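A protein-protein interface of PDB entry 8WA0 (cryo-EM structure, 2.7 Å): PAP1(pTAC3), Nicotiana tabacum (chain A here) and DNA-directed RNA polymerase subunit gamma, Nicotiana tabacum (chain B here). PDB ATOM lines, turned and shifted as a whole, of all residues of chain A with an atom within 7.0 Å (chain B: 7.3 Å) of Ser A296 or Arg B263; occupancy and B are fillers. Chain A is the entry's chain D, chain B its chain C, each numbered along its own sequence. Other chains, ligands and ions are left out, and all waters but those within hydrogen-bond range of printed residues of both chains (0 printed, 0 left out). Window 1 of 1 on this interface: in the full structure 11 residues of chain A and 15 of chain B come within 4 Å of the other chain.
Hydrophobic or aromatic side chains of chain A that line the printed part of chain B: Tyr A466.
Among the printed residues, no Asp or Glu carboxylate lies within 4 Å of a Lys or Arg side-chain nitrogen of the other chain.
NZ of Lys A454 touches O of Ile B266, 3.6 Å away.
CE1 of Tyr A466 touches O of Lys B259 (3.6 Å).
The backbone carbonyl oxygen (O) of Arg B263 lies close to the backbone carbonyl oxygen (O) of Ser A296 (2.9 Å).
The backbone carbonyl oxygen of Phe B261 is in hydrogen-bond range of the side-chain amino group of Lys A454 (3.0 Å).
Of the printed residues of chain B, Ser A296 touches Arg B263.
Printed residues of chain B within 4 Å of Lys A454: Phe B261 (3.0 Å) and Ile B266 (3.6 Å).
Of the printed residues of chain B, Tyr A466 touches Lys B259 (3.6 Å).
Of the printed residues of chain A, Lys B259 touches Tyr A466 (3.6 Å).
Printed residues of chain A within 4 Å of Phe B261: Lys A454 (3.0 Å).
Of chain A, only Ser A296 (2.9 Å) comes within 4 Å of Arg B263.
Of the printed residues of chain A, Ile B266 touches Lys A454.
The nearest residue of chain A that does not touch Arg B263 is Tyr A466 (4.1 Å).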
ATOM      1  N   GLY A 258      -7.686 -19.428  -3.827  1.00  0.00           N
ATOM      2  CA  GLY A 258      -7.744 -18.618  -5.023  1.00  0.00           C
ATOM      3  C   GLY A 258      -7.632 -17.169  -4.664  1.00  0.00           C
ATOM      4  O   GLY A 258      -7.299 -16.344  -5.506  1.00  0.00           O
ATOM      5  N   PRO A 260      -5.544 -14.760  -2.549  1.00  0.00           N
ATOM      6  CA  PRO A 260      -4.286 -14.746  -1.818  1.00  0.00           C
ATOM      7  C   PRO A 260      -4.383 -14.154  -0.435  1.00  0.00           C
ATOM      8  O   PRO A 260      -3.692 -14.625   0.454  1.00  0.00           O
ATOM      9  CB  PRO A 260      -3.408 -13.876  -2.688  1.00  0.00           C
ATOM     10  CG  PRO A 260      -3.950 -14.046  -4.057  1.00  0.00           C
ATOM     11  CD  PRO A 260      -5.429 -14.085  -3.848  1.00  0.00           C
ATOM     12  N   ALA A 294      -1.864 -17.675  -8.245  1.00  0.00           N
ATOM     13  CA  ALA A 294      -3.079 -16.871  -8.169  1.00  0.00           C
ATOM     14  C   ALA A 294      -3.395 -16.379  -9.556  1.00  0.00           C
ATOM     15  O   ALA A 294      -2.491 -16.060 -10.321  1.00  0.00           O
ATOM     16  CB  ALA A 294      -2.882 -15.700  -7.242  1.00  0.00           C
ATOM     17  N   GLU A 295      -4.670 -16.306  -9.895  1.00  0.00           N
ATOM     18  CA  GLU A 295      -5.035 -15.940 -11.261  1.00  0.00           C
ATOM     19  C   GLU A 295      -5.466 -14.519 -11.610  1.00  0.00           C
ATOM     20  O   GLU A 295      -5.829 -14.274 -12.753  1.00  0.00           O
ATOM     21  CB  GLU A 295      -6.134 -16.886 -11.746  1.00  0.00           C
ATOM     22  N   SER A 296      -5.451 -13.575 -10.678  1.00  0.00           N
ATOM     23  CA  SER A 296      -5.996 -12.266 -11.033  1.00  0.00           C
ATOM     24  C   SER A 296      -5.212 -10.959 -11.091  1.00  0.00           C
ATOM     25  O   SER A 296      -5.654 -10.049 -11.769  1.00  0.00           O
ATOM     26  CB  SER A 296      -7.265 -12.036 -10.231  1.00  0.00           C
ATOM     27  N   TYR A 297      -4.073 -10.830 -10.437  1.00  0.00           N
ATOM     28  CA  TYR A 297      -3.390  -9.533 -10.408  1.00  0.00           C
ATOM     29  C   TYR A 297      -1.885  -9.692 -10.406  1.00  0.00           C
ATOM     30  O   TYR A 297      -1.400 -10.812 -10.400  1.00  0.00           O
ATOM     31  CB  TYR A 297      -3.854  -8.693  -9.227  1.00  0.00           C
ATOM     32  CG  TYR A 297      -5.279  -8.200  -9.320  1.00  0.00           C
ATOM     33  CD1 TYR A 297      -5.605  -7.118 -10.120  1.00  0.00           C
ATOM     34  CD2 TYR A 297      -6.299  -8.821  -8.614  1.00  0.00           C
ATOM     35  CE1 TYR A 297      -6.906  -6.668 -10.217  1.00  0.00           C
ATOM     36  CE2 TYR A 297      -7.602  -8.379  -8.708  1.00  0.00           C
ATOM     37  CZ  TYR A 297      -7.897  -7.303  -9.509  1.00  0.00           C
ATOM     38  OH  TYR A 297      -9.189  -6.852  -9.607  1.00  0.00           O
ATOM     39  N   ASP A 298      -1.126  -8.601 -10.398  1.00  0.00           N
ATOM     40  CA  ASP A 298       0.336  -8.715 -10.528  1.00  0.00           C
ATOM     41  C   ASP A 298       1.049  -9.528  -9.459  1.00  0.00           C
ATOM     42  O   ASP A 298       1.932 -10.299  -9.792  1.00  0.00           O
ATOM     43  CB  ASP A 298       0.987  -7.341 -10.640  1.00  0.00           C
ATOM     44  N   ARG A 299       0.699  -9.376  -8.198  1.00  0.00           N
ATOM     45  CA  ARG A 299       1.265 -10.233  -7.158  1.00  0.00           C
ATOM     46  C   ARG A 299       2.719 -10.662  -7.287  1.00  0.00           C
ATOM     47  O   ARG A 299       3.013 -11.829  -7.093  1.00  0.00           O
ATOM     48  CB  ARG A 299       0.421 -11.503  -7.053  1.00  0.00           C
ATOM     49  CG  ARG A 299      -0.816 -11.410  -6.173  1.00  0.00           C
ATOM     50  CD  ARG A 299      -1.853 -10.450  -6.723  1.00  0.00           C
ATOM     51  NE  ARG A 299      -3.066 -10.397  -5.919  1.00  0.00           N
ATOM     52  CZ  ARG A 299      -4.160 -11.100  -6.181  1.00  0.00           C
ATOM     53  NH1 ARG A 299      -4.195 -11.914  -7.224  1.00  0.00           N
ATOM     54  NH2 ARG A 299      -5.221 -10.986  -5.401  1.00  0.00           N
ATOM     55  N   LYS A 454      -8.160 -12.045 -26.343  1.00  0.00           N
ATOM     56  CA  LYS A 454      -6.803 -11.942 -25.798  1.00  0.00           C
ATOM     57  C   LYS A 454      -6.211 -13.216 -25.214  1.00  0.00           C
ATOM     58  O   LYS A 454      -5.983 -13.304 -24.009  1.00  0.00           O
ATOM     59  CB  LYS A 454      -6.723 -10.797 -24.779  1.00  0.00           C
ATOM     60  CG  LYS A 454      -7.957 -10.640 -23.903  1.00  0.00           C
ATOM     61  CD  LYS A 454      -7.810  -9.468 -22.945  1.00  0.00           C
ATOM     62  CE  LYS A 454      -9.061  -9.287 -22.100  1.00  0.00           C
ATOM     63  NZ  LYS A 454      -8.955  -8.129 -21.173  1.00  0.00           N
ATOM     64  N   ILE A 465       2.633 -15.235 -17.361  1.00  0.00           N
ATOM     65  CA  ILE A 465       1.547 -14.371 -17.008  1.00  0.00           C
ATOM     66  C   ILE A 465       1.213 -13.332 -18.016  1.00  0.00           C
ATOM     67  O   ILE A 465       0.067 -13.184 -18.393  1.00  0.00           O
ATOM     68  CB  ILE A 465       1.907 -13.668 -15.700  1.00  0.00           C
ATOM     69  CG1 ILE A 465       2.164 -14.691 -14.599  1.00  0.00           C
ATOM     70  CG2 ILE A 465       0.826 -12.692 -15.278  1.00  0.00           C
ATOM     71  CD1 ILE A 465       0.944 -15.499 -14.220  1.00  0.00           C
ATOM     72  N   TYR A 466       2.204 -12.639 -18.514  1.00  0.00           N
ATOM     73  CA  TYR A 466       1.912 -11.568 -19.408  1.00  0.00           C
ATOM     74  C   TYR A 466       2.283 -11.962 -20.812  1.00  0.00           C
ATOM     75  O   TYR A 466       1.457 -11.833 -21.709  1.00  0.00           O
ATOM     76  CB  TYR A 466       2.661 -10.342 -18.938  1.00  0.00           C
ATOM     77  CG  TYR A 466       2.008  -9.608 -17.803  1.00  0.00           C
ATOM     78  CD1 TYR A 466       0.648  -9.363 -17.807  1.00  0.00           C
ATOM     79  CD2 TYR A 466       2.752  -9.142 -16.742  1.00  0.00           C
ATOM     80  CE1 TYR A 466       0.047  -8.686 -16.769  1.00  0.00           C
ATOM     81  CE2 TYR A 466       2.161  -8.463 -15.704  1.00  0.00           C
ATOM     82  CZ  TYR A 466       0.809  -8.239 -15.723  1.00  0.00           C
ATOM     83  OH  TYR A 466       0.214  -7.561 -14.688  1.00  0.00           O
ATOM     84  N   ALA B 258      -1.795  -0.986 -20.439  1.00  0.00           N
ATOM     85  CA  ALA B 258      -1.992  -2.212 -21.158  1.00  0.00           C
ATOM     86  C   ALA B 258      -1.822  -3.445 -20.315  1.00  0.00           C
ATOM     87  O   ALA B 258      -2.564  -4.397 -20.457  1.00  0.00           O
ATOM     88  CB  ALA B 258      -1.072  -2.236 -22.335  1.00  0.00           C
ATOM     89  N   LYS B 259      -0.837  -3.427 -19.433  1.00  0.00           N
ATOM     90  CA  LYS B 259      -0.590  -4.580 -18.598  1.00  0.00           C
ATOM     91  C   LYS B 259      -1.809  -4.856 -17.769  1.00  0.00           C
ATOM     92  O   LYS B 259      -2.215  -6.004 -17.608  1.00  0.00           O
ATOM     93  CB  LYS B 259       0.591  -4.335 -17.687  1.00  0.00           C
ATOM     94  CG  LYS B 259       1.906  -4.874 -18.211  1.00  0.00           C
ATOM     95  CD  LYS B 259       2.984  -4.777 -17.149  1.00  0.00           C
ATOM     96  CE  LYS B 259       4.275  -5.416 -17.620  1.00  0.00           C
ATOM     97  NZ  LYS B 259       5.307  -5.425 -16.548  1.00  0.00           N
ATOM     98  N   HIS B 260      -2.409  -3.799 -17.246  1.00  0.00           N
ATOM     99  CA  HIS B 260      -3.568  -3.973 -16.400  1.00  0.00           C
ATOM    100  C   HIS B 260      -4.652  -4.610 -17.211  1.00  0.00           C
ATOM    101  O   HIS B 260      -5.298  -5.530 -16.759  1.00  0.00           O
ATOM    102  CB  HIS B 260      -4.047  -2.643 -15.850  1.00  0.00           C
ATOM    103  CG  HIS B 260      -3.177  -2.094 -14.768  1.00  0.00           C
ATOM    104  ND1 HIS B 260      -2.917  -2.784 -13.605  1.00  0.00           N
ATOM    105  CD2 HIS B 260      -2.514  -0.920 -14.665  1.00  0.00           C
ATOM    106  CE1 HIS B 260      -2.125  -2.062 -12.836  1.00  0.00           C
ATOM    107  NE2 HIS B 260      -1.864  -0.926 -13.457  1.00  0.00           N
ATOM    108  N   PHE B 261      -4.805  -4.172 -18.445  1.00  0.00           N
ATOM    109  CA  PHE B 261      -5.859  -4.699 -19.280  1.00  0.00           C
ATOM    110  C   PHE B 261      -5.690  -6.188 -19.508  1.00  0.00           C
ATOM    111  O   PHE B 261      -6.673  -6.915 -19.579  1.00  0.00           O
ATOM    112  CB  PHE B 261      -5.938  -3.956 -20.602  1.00  0.00           C
ATOM    113  CG  PHE B 261      -6.849  -2.776 -20.574  1.00  0.00           C
ATOM    114  CD1 PHE B 261      -8.205  -2.947 -20.396  1.00  0.00           C
ATOM    115  CD2 PHE B 261      -6.355  -1.500 -20.742  1.00  0.00           C
ATOM    116  CE1 PHE B 261      -9.056  -1.865 -20.373  1.00  0.00           C
ATOM    117  CE2 PHE B 261      -7.197  -0.412 -20.720  1.00  0.00           C
ATOM    118  CZ  PHE B 261      -8.552  -0.595 -20.538  1.00  0.00           C
ATOM    119  N   ILE B 262      -4.454  -6.657 -19.585  1.00  0.00           N
ATOM    120  CA  ILE B 262      -4.221  -8.072 -19.845  1.00  0.00           C
ATOM    121  C   ILE B 262      -4.749  -8.916 -18.698  1.00  0.00           C
ATOM    122  O   ILE B 262      -5.379  -9.947 -18.920  1.00  0.00           O
ATOM    123  CB  ILE B 262      -2.736  -8.377 -20.087  1.00  0.00           C
ATOM    124  CG1 ILE B 262      -2.215  -7.564 -21.265  1.00  0.00           C
ATOM    125  CG2 ILE B 262      -2.521  -9.854 -20.367  1.00  0.00           C
ATOM    126  CD1 ILE B 262      -0.740  -7.759 -21.527  1.00  0.00           C
ATOM    127  N   ARG B 263      -4.529  -8.472 -17.470  1.00  0.00           N
ATOM    128  CA  ARG B 263      -4.943  -9.261 -16.319  1.00  0.00           C
ATOM    129  C   ARG B 263      -6.174  -8.759 -15.568  1.00  0.00           C
ATOM    130  O   ARG B 263      -6.395  -9.164 -14.433  1.00  0.00           O
ATOM    131  CB  ARG B 263      -3.778  -9.443 -15.356  1.00  0.00           C
ATOM    132  N   THR B 264      -6.979  -7.881 -16.157  1.00  0.00           N
ATOM    133  CA  THR B 264      -8.089  -7.315 -15.386  1.00  0.00           C
ATOM    134  C   THR B 264      -9.524  -7.643 -15.753  1.00  0.00           C
ATOM    135  O   THR B 264     -10.427  -7.238 -15.039  1.00  0.00           O
ATOM    136  CB  THR B 264      -7.991  -5.784 -15.293  1.00  0.00           C
ATOM    137  OG1 THR B 264      -8.769  -5.312 -14.187  1.00  0.00           O
ATOM    138  CG2 THR B 264      -8.476  -5.124 -16.575  1.00  0.00           C
ATOM    139  N   ASN B 265      -9.750  -8.354 -16.843  1.00  0.00           N
ATOM    140  CA  ASN B 265     -11.121  -8.754 -17.245  1.00  0.00           C
ATOM    141  C   ASN B 265     -12.028  -7.610 -17.740  1.00  0.00           C
ATOM    142  O   ASN B 265     -13.207  -7.805 -18.004  1.00  0.00           O
ATOM    143  CB  ASN B 265     -11.767  -9.741 -16.239  1.00  0.00           C
ATOM    144  N   ILE B 266     -11.458  -6.435 -17.957  1.00  0.00           N
ATOM    145  CA  ILE B 266     -12.226  -5.315 -18.478  1.00  0.00           C
ATOM    146  C   ILE B 266     -11.809  -5.147 -19.926  1.00  0.00           C
ATOM    147  O   ILE B 266     -10.620  -5.091 -20.212  1.00  0.00           O
ATOM    148  CB  ILE B 266     -11.906  -4.022 -17.714  1.00  0.00           C
ATOM    149  CG1 ILE B 266     -12.274  -4.163 -16.239  1.00  0.00           C
ATOM    150  CG2 ILE B 266     -12.639  -2.835 -18.315  1.00  0.00           C
ATOM    151  CD1 ILE B 266     -13.759  -4.307 -16.004  1.00  0.00           C
